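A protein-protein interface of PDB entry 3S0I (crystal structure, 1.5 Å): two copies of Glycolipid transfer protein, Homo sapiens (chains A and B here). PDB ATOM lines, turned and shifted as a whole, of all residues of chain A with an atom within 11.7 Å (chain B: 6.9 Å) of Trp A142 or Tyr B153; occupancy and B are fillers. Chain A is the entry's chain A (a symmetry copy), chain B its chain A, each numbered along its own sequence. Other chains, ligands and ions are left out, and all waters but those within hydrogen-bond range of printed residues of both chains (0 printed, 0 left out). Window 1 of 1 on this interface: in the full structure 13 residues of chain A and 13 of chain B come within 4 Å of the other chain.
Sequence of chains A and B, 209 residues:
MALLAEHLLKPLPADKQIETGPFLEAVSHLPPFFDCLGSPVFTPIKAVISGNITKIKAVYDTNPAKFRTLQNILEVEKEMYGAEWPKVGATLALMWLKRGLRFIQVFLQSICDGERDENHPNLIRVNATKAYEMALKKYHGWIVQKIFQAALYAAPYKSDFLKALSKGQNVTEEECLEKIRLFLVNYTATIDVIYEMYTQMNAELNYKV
6 positions are printed for both chains.
Of the 8 pairs that touch across the chains among the printed residues, none has its exchanged pair printed and touching as well.
Printed residues of chain A that touch a printed residue of chain B: Trp A142, Ile A143, Val A144 and Ile A147.
Hydrophobic or aromatic side chains of chain A that line the printed part of chain B: Trp A142, Ile A143, Val A144 and Ile A147.
Of the 13 printed residues of chain B, 4 touch a printed residue of chain A.
Hydrophobic or aromatic side chains of chain B within 4 Å of the printed part of chain A: Val B41, Ala B150, Tyr B153 and Ala B154.
Among the printed residues, no Asp or Glu carboxylate lies within 4 Å of a Lys or Arg side-chain nitrogen of the other chain.
Tyr B153 touches Trp A142.
CG2 of Ile A143 touches CG2 of Val B41 (3.7 Å).
Ile A143 touches Ala B150 (CG2 to O, 3.7 Å).
Ile A143 touches Tyr B153 (CD1 to C, 3.97 Å).
CD1 of Ile A143 touches CA of Ala B154, at 3.8 Å.
Val A144 touches Val B41.
Val B41 touches Ile A147.
CG1 of Ile A147 touches CB of Ala B150, at 3.9 Å.
His A140 touches none of the printed residues of chain B.
Trp A142 touches one residue of chain B.
Of the printed residues of chain B, Ile A143 touches Val B41 (3.7 Å), Ala B150 (3.7 Å), Tyr B153 (3.97 Å) and Ala B154 (3.8 Å).
Printed residues of chain B within 4 Å of Val A144: Val B41 (3.8 Å).
Of the printed residues of chain B, Ile A147 touches Val B41 (3.6 Å) and Ala B150 (3.9 Å).
Of the printed residues of chain A, Val B41 touches Ile A143, Val A144 and Ile A147.
No residue of chain A comes within 4 Å of Gln B149.
Of chain A, only Trp A142 and Ile A143 come within 4 Å of Tyr B153.
Ala B154 touches just one residue of chain A: Ile A143.
No residue of chain A comes within 4 Å of Ala B155.
The nearest residue of chain A that does not touch Tyr B153 is Lys A146 (5.5 Å).
The nearest printed residue of chain B that does not touch Ile A143 is Ala B151 (5.0 Å).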
ATOM      1  N   TYR A 132       9.986 -30.360 -11.994  1.00  0.00           N
ATOM      2  CA  TYR A 132       9.303 -29.097 -12.208  1.00  0.00           C
ATOM      3  C   TYR A 132       8.273 -28.843 -11.099  1.00  0.00           C
ATOM      4  O   TYR A 132       8.232 -27.758 -10.489  1.00  0.00           O
ATOM      5  CB  TYR A 132       8.647 -29.077 -13.589  1.00  0.00           C
ATOM      6  CG  TYR A 132       7.978 -27.768 -13.904  1.00  0.00           C
ATOM      7  CD1 TYR A 132       8.742 -26.606 -14.119  1.00  0.00           C
ATOM      8  CD2 TYR A 132       6.585 -27.678 -13.996  1.00  0.00           C
ATOM      9  CE1 TYR A 132       8.128 -25.401 -14.441  1.00  0.00           C
ATOM     10  CE2 TYR A 132       5.962 -26.473 -14.300  1.00  0.00           C
ATOM     11  CZ  TYR A 132       6.735 -25.339 -14.506  1.00  0.00           C
ATOM     12  OH  TYR A 132       6.114 -24.146 -14.802  1.00  0.00           O
ATOM     13  N   LEU A 136       9.792 -25.658  -9.142  1.00  0.00           N
ATOM     14  CA  LEU A 136       9.519 -24.423  -9.899  1.00  0.00           C
ATOM     15  C   LEU A 136       8.052 -24.067 -10.031  1.00  0.00           C
ATOM     16  O   LEU A 136       7.684 -22.883 -10.007  1.00  0.00           O
ATOM     17  CB  LEU A 136      10.135 -24.492 -11.302  1.00  0.00           C
ATOM     18  CG  LEU A 136      11.667 -24.491 -11.379  1.00  0.00           C
ATOM     19  CD1 LEU A 136      12.166 -24.873 -12.773  1.00  0.00           C
ATOM     20  CD2 LEU A 136      12.207 -23.130 -10.955  1.00  0.00           C
ATOM     21  N   LYS A 137       7.216 -25.087 -10.188  1.00  0.00           N
ATOM     22  CA  LYS A 137       5.816 -24.849 -10.578  1.00  0.00           C
ATOM     23  C   LYS A 137       5.067 -23.874  -9.657  1.00  0.00           C
ATOM     24  O   LYS A 137       4.272 -23.080 -10.133  1.00  0.00           O
ATOM     25  CB  LYS A 137       5.072 -26.167 -10.700  1.00  0.00           C
ATOM     26  CG  LYS A 137       3.645 -26.012 -11.193  1.00  0.00           C
ATOM     27  CD  LYS A 137       2.926 -27.338 -11.096  1.00  0.00           C
ATOM     28  CE  LYS A 137       1.474 -27.191 -11.495  1.00  0.00           C
ATOM     29  NZ  LYS A 137       0.850 -28.533 -11.592  1.00  0.00           N
ATOM     30  N   LYS A 138       5.354 -23.924  -8.352  1.00  0.00           N
ATOM     31  CA  LYS A 138       4.735 -23.062  -7.337  1.00  0.00           C
ATOM     32  C   LYS A 138       4.880 -21.574  -7.688  1.00  0.00           C
ATOM     33  O   LYS A 138       4.046 -20.756  -7.290  1.00  0.00           O
ATOM     34  CB  LYS A 138       5.386 -23.330  -5.954  1.00  0.00           C
ATOM     35  CG  LYS A 138       4.755 -22.612  -4.760  1.00  0.00           C
ATOM     36  CD  LYS A 138       5.354 -23.051  -3.420  1.00  0.00           C
ATOM     37  CE  LYS A 138       4.687 -22.319  -2.255  1.00  0.00           C
ATOM     38  NZ  LYS A 138       5.341 -22.525  -0.924  1.00  0.00           N
ATOM     39  N   TYR A 139       5.938 -21.242  -8.432  1.00  0.00           N
ATOM     40  CA  TYR A 139       6.328 -19.846  -8.694  1.00  0.00           C
ATOM     41  C   TYR A 139       6.042 -19.442 -10.131  1.00  0.00           C
ATOM     42  O   TYR A 139       6.475 -18.376 -10.564  1.00  0.00           O
ATOM     43  CB  TYR A 139       7.830 -19.636  -8.373  1.00  0.00           C
ATOM     44  CG  TYR A 139       8.199 -20.307  -7.073  1.00  0.00           C
ATOM     45  CD1 TYR A 139       7.751 -19.799  -5.857  1.00  0.00           C
ATOM     46  CD2 TYR A 139       8.934 -21.489  -7.065  1.00  0.00           C
ATOM     47  CE1 TYR A 139       8.042 -20.443  -4.659  1.00  0.00           C
ATOM     48  CE2 TYR A 139       9.224 -22.137  -5.888  1.00  0.00           C
ATOM     49  CZ  TYR A 139       8.788 -21.611  -4.691  1.00  0.00           C
ATOM     50  OH  TYR A 139       9.085 -22.282  -3.527  1.00  0.00           O
ATOM     51  N   HIS A 140       5.332 -20.304 -10.862  1.00  0.00           N
ATOM     52  CA  HIS A 140       5.009 -20.066 -12.264  1.00  0.00           C
ATOM     53  C   HIS A 140       3.534 -19.942 -12.518  1.00  0.00           C
ATOM     54  O   HIS A 140       2.750 -20.814 -12.117  1.00  0.00           O
ATOM     55  CB  HIS A 140       5.551 -21.192 -13.131  1.00  0.00           C
ATOM     56  CG  HIS A 140       7.043 -21.169 -13.308  1.00  0.00           C
ATOM     57  ND1 HIS A 140       7.697 -22.129 -13.990  1.00  0.00           N
ATOM     58  CD2 HIS A 140       8.020 -20.242 -12.887  1.00  0.00           C
ATOM     59  CE1 HIS A 140       9.009 -21.842 -14.013  1.00  0.00           C
ATOM     60  NE2 HIS A 140       9.204 -20.687 -13.338  1.00  0.00           N
ATOM     61  N   GLY A 141       3.156 -18.856 -13.203  1.00  0.00           N
ATOM     62  CA  GLY A 141       1.800 -18.657 -13.690  1.00  0.00           C
ATOM     63  C   GLY A 141       1.537 -19.477 -14.935  1.00  0.00           C
ATOM     64  O   GLY A 141       2.406 -20.217 -15.420  1.00  0.00           O
ATOM     65  N   TRP A 142       0.340 -19.312 -15.488  1.00  0.00           N
ATOM     66  CA  TRP A 142      -0.137 -20.163 -16.569  1.00  0.00           C
ATOM     67  C   TRP A 142       0.717 -20.112 -17.822  1.00  0.00           C
ATOM     68  O   TRP A 142       0.993 -21.155 -18.434  1.00  0.00           O
ATOM     69  CB  TRP A 142      -1.604 -19.848 -16.853  1.00  0.00           C
ATOM     70  CG  TRP A 142      -2.198 -20.647 -17.986  1.00  0.00           C
ATOM     71  CD1 TRP A 142      -2.841 -21.885 -17.919  1.00  0.00           C
ATOM     72  CD2 TRP A 142      -2.227 -20.273 -19.408  1.00  0.00           C
ATOM     73  NE1 TRP A 142      -3.244 -22.294 -19.165  1.00  0.00           N
ATOM     74  CE2 TRP A 142      -2.906 -21.374 -20.107  1.00  0.00           C
ATOM     75  CE3 TRP A 142      -1.774 -19.183 -20.144  1.00  0.00           C
ATOM     76  CZ2 TRP A 142      -3.102 -21.358 -21.486  1.00  0.00           C
ATOM     77  CZ3 TRP A 142      -1.985 -19.175 -21.534  1.00  0.00           C
ATOM     78  CH2 TRP A 142      -2.632 -20.239 -22.185  1.00  0.00           C
ATOM     79  N   ILE A 143       1.166 -18.916 -18.206  1.00  0.00           N
ATOM     80  CA  ILE A 143       2.005 -18.759 -19.413  1.00  0.00           C
ATOM     81  C   ILE A 143       3.365 -19.465 -19.293  1.00  0.00           C
ATOM     82  O   ILE A 143       3.789 -20.198 -20.207  1.00  0.00           O
ATOM     83  CB  ILE A 143       2.203 -17.270 -19.813  1.00  0.00           C
ATOM     84  CG1 ILE A 143       0.846 -16.589 -20.010  1.00  0.00           C
ATOM     85  CG2 ILE A 143       3.050 -17.161 -21.084  1.00  0.00           C
ATOM     86  CD1 ILE A 143       0.925 -15.085 -20.152  1.00  0.00           C
ATOM     87  N   VAL A 144       4.068 -19.239 -18.182  1.00  0.00           N
ATOM     88  CA  VAL A 144       5.358 -19.887 -17.988  1.00  0.00           C
ATOM     89  C   VAL A 144       5.190 -21.413 -17.979  1.00  0.00           C
ATOM     90  O   VAL A 144       6.018 -22.149 -18.562  1.00  0.00           O
ATOM     91  CB  VAL A 144       6.068 -19.322 -16.734  1.00  0.00           C
ATOM     92  CG1 VAL A 144       7.339 -20.089 -16.408  1.00  0.00           C
ATOM     93  CG2 VAL A 144       6.418 -17.856 -16.963  1.00  0.00           C
ATOM     94  N   GLN A 145       4.101 -21.891 -17.375  1.00  0.00           N
ATOM     95  CA  GLN A 145       3.821 -23.340 -17.373  1.00  0.00           C
ATOM     96  C   GLN A 145       3.655 -23.888 -18.799  1.00  0.00           C
ATOM     97  O   GLN A 145       4.156 -24.974 -19.112  1.00  0.00           O
ATOM     98  CB  GLN A 145       2.599 -23.679 -16.501  1.00  0.00           C
ATOM     99  CG  GLN A 145       2.827 -23.464 -15.009  1.00  0.00           C
ATOM    100  CD  GLN A 145       1.743 -24.061 -14.130  1.00  0.00           C
ATOM    101  OE1 GLN A 145       1.151 -25.105 -14.448  1.00  0.00           O
ATOM    102  NE2 GLN A 145       1.488 -23.413 -12.997  1.00  0.00           N
ATOM    103  N   LYS A 146       2.993 -23.120 -19.670  1.00  0.00           N
ATOM    104  CA  LYS A 146       2.842 -23.523 -21.065  1.00  0.00           C
ATOM    105  C   LYS A 146       4.191 -23.545 -21.767  1.00  0.00           C
ATOM    106  O   LYS A 146       4.453 -24.429 -22.584  1.00  0.00           O
ATOM    107  CB  LYS A 146       1.848 -22.624 -21.805  1.00  0.00           C
ATOM    108  CG  LYS A 146       0.392 -22.811 -21.378  1.00  0.00           C
ATOM    109  CD  LYS A 146      -0.190 -24.132 -21.879  1.00  0.00           C
ATOM    110  CE  LYS A 146      -1.439 -24.529 -21.103  1.00  0.00           C
ATOM    111  NZ  LYS A 146      -1.969 -25.865 -21.501  1.00  0.00           N
ATOM    112  N   ILE A 147       5.064 -22.604 -21.418  1.00  0.00           N
ATOM    113  CA  ILE A 147       6.424 -22.579 -21.960  1.00  0.00           C
ATOM    114  C   ILE A 147       7.232 -23.811 -21.544  1.00  0.00           C
ATOM    115  O   ILE A 147       7.948 -24.380 -22.374  1.00  0.00           O
ATOM    116  CB  ILE A 147       7.176 -21.290 -21.588  1.00  0.00           C
ATOM    117  CG1 ILE A 147       6.520 -20.090 -22.281  1.00  0.00           C
ATOM    118  CG2 ILE A 147       8.658 -21.397 -21.945  1.00  0.00           C
ATOM    119  CD1 ILE A 147       6.846 -18.762 -21.641  1.00  0.00           C
ATOM    120  N   PHE A 148       7.121 -24.207 -20.269  1.00  0.00           N
ATOM    121  CA  PHE A 148       7.734 -25.453 -19.792  1.00  0.00           C
ATOM    122  C   PHE A 148       7.296 -26.639 -20.657  1.00  0.00           C
ATOM    123  O   PHE A 148       8.130 -27.446 -21.108  1.00  0.00           O
ATOM    124  CB  PHE A 148       7.401 -25.714 -18.306  1.00  0.00           C
ATOM    125  CG  PHE A 148       7.749 -27.107 -17.840  1.00  0.00           C
ATOM    126  CD1 PHE A 148       9.076 -27.500 -17.692  1.00  0.00           C
ATOM    127  CD2 PHE A 148       6.740 -28.045 -17.583  1.00  0.00           C
ATOM    128  CE1 PHE A 148       9.391 -28.797 -17.277  1.00  0.00           C
ATOM    129  CE2 PHE A 148       7.052 -29.335 -17.171  1.00  0.00           C
ATOM    130  CZ  PHE A 148       8.379 -29.714 -17.027  1.00  0.00           C
ATOM    131  N   GLN A 149       5.987 -26.738 -20.884  1.00  0.00           N
ATOM    132  CA  GLN A 149       5.413 -27.800 -21.728  1.00  0.00           C
ATOM    133  C   GLN A 149       6.015 -27.845 -23.130  1.00  0.00           C
ATOM    134  O   GLN A 149       6.322 -28.935 -23.640  1.00  0.00           O
ATOM    135  CB  GLN A 149       3.887 -27.685 -21.795  1.00  0.00           C
ATOM    136  CG  GLN A 149       3.184 -28.065 -20.494  1.00  0.00           C
ATOM    137  CD  GLN A 149       1.715 -27.657 -20.452  1.00  0.00           C
ATOM    138  OE1 GLN A 149       1.025 -27.635 -21.476  1.00  0.00           O
ATOM    139  NE2 GLN A 149       1.230 -27.339 -19.255  1.00  0.00           N
ATOM    140  N   ALA A 150       6.189 -26.672 -23.744  1.00  0.00           N
ATOM    141  CA  ALA A 150       6.816 -26.570 -25.062  1.00  0.00           C
ATOM    142  C   ALA A 150       8.278 -27.020 -25.035  1.00  0.00           C
ATOM    143  O   ALA A 150       8.714 -27.798 -25.896  1.00  0.00           O
ATOM    144  CB  ALA A 150       6.699 -25.152 -25.601  1.00  0.00           C
ATOM    145  N   ALA A 151       9.024 -26.552 -24.031  1.00  0.00           N
ATOM    146  CA  ALA A 151      10.444 -26.881 -23.898  1.00  0.00           C
ATOM    147  C   ALA A 151      10.681 -28.385 -23.732  1.00  0.00           C
ATOM    148  O   ALA A 151      11.681 -28.922 -24.225  1.00  0.00           O
ATOM    149  CB  ALA A 151      11.066 -26.109 -22.742  1.00  0.00           C
ATOM    150  N   TYR A 153       9.322 -30.831 -25.198  1.00  0.00           N
ATOM    151  CA  TYR A 153       9.411 -31.523 -26.478  1.00  0.00           C
ATOM    152  C   TYR A 153      10.864 -31.623 -26.927  1.00  0.00           C
ATOM    153  O   TYR A 153      11.229 -32.540 -27.644  1.00  0.00           O
ATOM    154  CB  TYR A 153       8.558 -30.828 -27.552  1.00  0.00           C
ATOM    155  CG  TYR A 153       7.104 -30.581 -27.160  1.00  0.00           C
ATOM    156  CD1 TYR A 153       6.448 -29.406 -27.543  1.00  0.00           C
ATOM    157  CD2 TYR A 153       6.390 -31.515 -26.399  1.00  0.00           C
ATOM    158  CE1 TYR A 153       5.122 -29.175 -27.188  1.00  0.00           C
ATOM    159  CE2 TYR A 153       5.068 -31.290 -26.035  1.00  0.00           C
ATOM    160  CZ  TYR A 153       4.437 -30.122 -26.432  1.00  0.00           C
ATOM    161  OH  TYR A 153       3.123 -29.903 -26.074  1.00  0.00           O
ATOM    162  N   TYR A 207       5.876 -15.156  -4.648  1.00  0.00           N
ATOM    163  CA  TYR A 207       5.256 -14.568  -5.839  1.00  0.00           C
ATOM    164  C   TYR A 207       5.454 -15.439  -7.092  1.00  0.00           C
ATOM    165  O   TYR A 207       6.436 -16.210  -7.184  1.00  0.00           O
ATOM    166  CB  TYR A 207       5.747 -13.131  -6.068  1.00  0.00           C
ATOM    167  CG  TYR A 207       7.163 -13.005  -6.560  1.00  0.00           C
ATOM    168  CD1 TYR A 207       7.441 -12.990  -7.934  1.00  0.00           C
ATOM    169  CD2 TYR A 207       8.234 -12.885  -5.660  1.00  0.00           C
ATOM    170  CE1 TYR A 207       8.749 -12.859  -8.398  1.00  0.00           C
ATOM    171  CE2 TYR A 207       9.553 -12.765  -6.118  1.00  0.00           C
ATOM    172  CZ  TYR A 207       9.792 -12.756  -7.483  1.00  0.00           C
ATOM    173  OH  TYR A 207      11.059 -12.605  -7.946  1.00  0.00           O
ATOM    174  N   LYS A 208       4.501 -15.334  -8.022  1.00  0.00           N
ATOM    175  CA  LYS A 208       4.582 -16.048  -9.292  1.00  0.00           C
ATOM    176  C   LYS A 208       5.041 -15.139 -10.413  1.00  0.00           C
ATOM    177  O   LYS A 208       4.761 -13.941 -10.407  1.00  0.00           O
ATOM    178  CB  LYS A 208       3.243 -16.684  -9.687  1.00  0.00           C
ATOM    179  CG  LYS A 208       2.739 -17.742  -8.722  1.00  0.00           C
ATOM    180  CD  LYS A 208       1.601 -18.518  -9.350  1.00  0.00           C
ATOM    181  CE  LYS A 208       1.091 -19.591  -8.419  1.00  0.00           C
ATOM    182  NZ  LYS A 208      -0.028 -20.304  -9.080  1.00  0.00           N
ATOM    183  N   VAL A 209       5.733 -15.722 -11.384  1.00  0.00           N
ATOM    184  CA  VAL A 209       6.083 -15.002 -12.600  1.00  0.00           C
ATOM    185  C   VAL A 209       5.136 -15.362 -13.739  1.00  0.00           C
ATOM    186  O   VAL A 209       4.635 -16.485 -13.783  1.00  0.00           O
ATOM    187  CB  VAL A 209       7.563 -15.209 -13.010  1.00  0.00           C
ATOM    188  CG1 VAL A 209       8.486 -14.533 -12.004  1.00  0.00           C
ATOM    189  CG2 VAL A 209       7.924 -16.677 -13.173  1.00  0.00           C
ATOM    190  OXT VAL A 209       4.850 -14.540 -14.624  1.00  0.00           O
ATOM    191  N   VAL B  41       7.894 -13.375 -18.402  1.00  0.00           N
ATOM    192  CA  VAL B  41       8.000 -14.333 -19.497  1.00  0.00           C
ATOM    193  C   VAL B  41       9.155 -13.967 -20.448  1.00  0.00           C
ATOM    194  O   VAL B  41       9.804 -14.843 -21.034  1.00  0.00           O
ATOM    195  CB  VAL B  41       6.661 -14.414 -20.254  1.00  0.00           C
ATOM    196  CG1 VAL B  41       6.793 -15.125 -21.592  1.00  0.00           C
ATOM    197  CG2 VAL B  41       5.616 -15.099 -19.379  1.00  0.00           C
ATOM    198  N   PHE B  42       9.416 -12.669 -20.585  1.00  0.00           N
ATOM    199  CA  PHE B  42      10.440 -12.186 -21.526  1.00  0.00           C
ATOM    200  C   PHE B  42      11.838 -12.127 -20.964  1.00  0.00           C
ATOM    201  O   PHE B  42      12.777 -11.823 -21.683  1.00  0.00           O
ATOM    202  CB  PHE B  42      10.036 -10.833 -22.131  1.00  0.00           C
ATOM    203  CG  PHE B  42       8.705 -10.884 -22.795  1.00  0.00           C
ATOM    204  CD1 PHE B  42       8.507 -11.688 -23.920  1.00  0.00           C
ATOM    205  CD2 PHE B  42       7.606 -10.237 -22.227  1.00  0.00           C
ATOM    206  CE1 PHE B  42       7.256 -11.782 -24.516  1.00  0.00           C
ATOM    207  CE2 PHE B  42       6.363 -10.323 -22.824  1.00  0.00           C
ATOM    208  CZ  PHE B  42       6.181 -11.102 -23.963  1.00  0.00           C
ATOM    209  N   ARG B 125      -0.346  -8.065 -31.199  1.00  0.00           N
ATOM    210  CA  ARG B 125      -0.046  -9.422 -31.668  1.00  0.00           C
ATOM    211  C   ARG B 125       0.305  -9.461 -33.155  1.00  0.00           C
ATOM    212  O   ARG B 125       1.325 -10.050 -33.554  1.00  0.00           O
ATOM    213  CB  ARG B 125      -1.216 -10.374 -31.358  1.00  0.00           C
ATOM    214  CG  ARG B 125      -1.289 -10.886 -29.920  1.00  0.00           C
ATOM    215  CD  ARG B 125      -2.457 -11.859 -29.737  1.00  0.00           C
ATOM    216  NE  ARG B 125      -2.595 -12.759 -30.886  1.00  0.00           N
ATOM    217  CZ  ARG B 125      -2.270 -14.051 -30.906  1.00  0.00           C
ATOM    218  NH1 ARG B 125      -2.431 -14.743 -32.026  1.00  0.00           N
ATOM    219  NH2 ARG B 125      -1.800 -14.661 -29.820  1.00  0.00           N
ATOM    220  N   LYS B 146       6.815 -22.923 -31.594  1.00  0.00           N
ATOM    221  CA  LYS B 146       5.775 -23.134 -30.591  1.00  0.00           C
ATOM    222  C   LYS B 146       6.037 -22.281 -29.359  1.00  0.00           C
ATOM    223  O   LYS B 146       5.103 -21.744 -28.763  1.00  0.00           O
ATOM    224  CB  LYS B 146       5.642 -24.614 -30.222  1.00  0.00           C
ATOM    225  CG  LYS B 146       5.043 -25.486 -31.324  1.00  0.00           C
ATOM    226  CD  LYS B 146       3.547 -25.236 -31.507  1.00  0.00           C
ATOM    227  CE  LYS B 146       3.052 -25.738 -32.857  1.00  0.00           C
ATOM    228  NZ  LYS B 146       1.617 -25.416 -33.105  1.00  0.00           N
ATOM    229  N   PHE B 148       7.593 -19.307 -29.381  1.00  0.00           N
ATOM    230  CA  PHE B 148       7.166 -17.965 -29.797  1.00  0.00           C
ATOM    231  C   PHE B 148       5.662 -17.781 -29.570  1.00  0.00           C
ATOM    232  O   PHE B 148       5.221 -16.771 -28.991  1.00  0.00           O
ATOM    233  CB  PHE B 148       7.530 -17.688 -31.273  1.00  0.00           C
ATOM    234  CG  PHE B 148       6.866 -16.458 -31.842  1.00  0.00           C
ATOM    235  CD1 PHE B 148       7.247 -15.185 -31.429  1.00  0.00           C
ATOM    236  CD2 PHE B 148       5.826 -16.576 -32.774  1.00  0.00           C
ATOM    237  CE1 PHE B 148       6.616 -14.050 -31.948  1.00  0.00           C
ATOM    238  CE2 PHE B 148       5.198 -15.449 -33.289  1.00  0.00           C
ATOM    239  CZ  PHE B 148       5.586 -14.186 -32.869  1.00  0.00           C
ATOM    240  N   GLN B 149       4.883 -18.758 -30.031  1.00  0.00           N
ATOM    241  CA  GLN B 149       3.421 -18.745 -29.857  1.00  0.00           C
ATOM    242  C   GLN B 149       2.990 -18.612 -28.398  1.00  0.00           C
ATOM    243  O   GLN B 149       2.067 -17.839 -28.091  1.00  0.00           O
ATOM    244  CB  GLN B 149       2.779 -19.977 -30.503  1.00  0.00           C
ATOM    245  CG  GLN B 149       2.797 -19.950 -32.029  1.00  0.00           C
ATOM    246  CD  GLN B 149       2.454 -21.293 -32.667  1.00  0.00           C
ATOM    247  OE1 GLN B 149       1.665 -22.077 -32.130  1.00  0.00           O
ATOM    248  NE2 GLN B 149       3.044 -21.557 -33.830  1.00  0.00           N
ATOM    249  N   ALA B 150       3.655 -19.353 -27.508  1.00  0.00           N
ATOM    250  CA  ALA B 150       3.385 -19.270 -26.073  1.00  0.00           C
ATOM    251  C   ALA B 150       3.728 -17.890 -25.506  1.00  0.00           C
ATOM    252  O   ALA B 150       2.930 -17.299 -24.764  1.00  0.00           O
ATOM    253  CB  ALA B 150       4.138 -20.360 -25.325  1.00  0.00           C
ATOM    254  N   ALA B 151       4.899 -17.370 -25.879  1.00  0.00           N
ATOM    255  CA  ALA B 151       5.364 -16.070 -25.393  1.00  0.00           C
ATOM    256  C   ALA B 151       4.422 -14.929 -25.790  1.00  0.00           C
ATOM    257  O   ALA B 151       4.239 -13.970 -25.029  1.00  0.00           O
ATOM    258  CB  ALA B 151       6.779 -15.792 -25.878  1.00  0.00           C
ATOM    259  N   LEU B 152       3.823 -15.062 -26.973  1.00  0.00           N
ATOM    260  CA  LEU B 152       2.863 -14.089 -27.501  1.00  0.00           C
ATOM    261  C   LEU B 152       1.728 -13.787 -26.534  1.00  0.00           C
ATOM    262  O   LEU B 152       1.294 -12.636 -26.431  1.00  0.00           O
ATOM    263  CB  LEU B 152       2.277 -14.554 -28.843  1.00  0.00           C
ATOM    264  CG  LEU B 152       2.755 -13.875 -30.130  1.00  0.00           C
ATOM    265  CD1 LEU B 152       1.980 -14.403 -31.329  1.00  0.00           C
ATOM    266  CD2 LEU B 152       2.622 -12.360 -30.040  1.00  0.00           C
ATOM    267  N   TYR B 153       1.266 -14.810 -25.810  1.00  0.00           N
ATOM    268  CA  TYR B 153       0.174 -14.635 -24.860  1.00  0.00           C
ATOM    269  C   TYR B 153       0.546 -13.594 -23.810  1.00  0.00           C
ATOM    270  O   TYR B 153      -0.320 -12.936 -23.258  1.00  0.00           O
ATOM    271  CB  TYR B 153      -0.208 -15.967 -24.192  1.00  0.00           C
ATOM    272  CG  TYR B 153      -0.497 -17.112 -25.157  1.00  0.00           C
ATOM    273  CD1 TYR B 153      -0.098 -18.419 -24.859  1.00  0.00           C
ATOM    274  CD2 TYR B 153      -1.159 -16.887 -26.371  1.00  0.00           C
ATOM    275  CE1 TYR B 153      -0.359 -19.468 -25.736  1.00  0.00           C
ATOM    276  CE2 TYR B 153      -1.418 -17.927 -27.255  1.00  0.00           C
ATOM    277  CZ  TYR B 153      -1.020 -19.215 -26.935  1.00  0.00           C
ATOM    278  OH  TYR B 153      -1.282 -20.247 -27.812  1.00  0.00           O
ATOM    279  N   ALA B 154       1.844 -13.425 -23.570  1.00  0.00           N
ATOM    280  CA  ALA B 154       2.323 -12.486 -22.556  1.00  0.00           C
ATOM    281  C   ALA B 154       2.541 -11.057 -23.063  1.00  0.00           C
ATOM    282  O   ALA B 154       2.936 -10.175 -22.289  1.00  0.00           O
ATOM    283  CB  ALA B 154       3.599 -13.012 -21.928  1.00  0.00           C
ATOM    284  N   ALA B 155       2.318 -10.835 -24.353  1.00  0.00           N
ATOM    285  CA  ALA B 155       2.535  -9.514 -24.952  1.00  0.00           C
ATOM    286  C   ALA B 155       1.680  -8.447 -24.249  1.00  0.00           C
ATOM    287  O   ALA B 155       0.526  -8.711 -23.897  1.00  0.00           O
ATOM    288  CB  ALA B 155       2.222  -9.561 -26.439  1.00  0.00           C
ATOM    289  N   PRO B 156       2.255  -7.248 -24.007  1.00  0.00           N
ATOM    290  CA  PRO B 156       1.472  -6.186 -23.341  1.00  0.00           C
ATOM    291  C   PRO B 156       0.372  -5.632 -24.219  1.00  0.00           C
ATOM    292  O   PRO B 156       0.425  -5.773 -25.442  1.00  0.00           O
ATOM    293  CB  PRO B 156       2.502  -5.077 -23.095  1.00  0.00           C
ATOM    294  CG  PRO B 156       3.588  -5.329 -24.094  1.00  0.00           C
ATOM    295  CD  PRO B 156       3.643  -6.826 -24.273  1.00  0.00           C
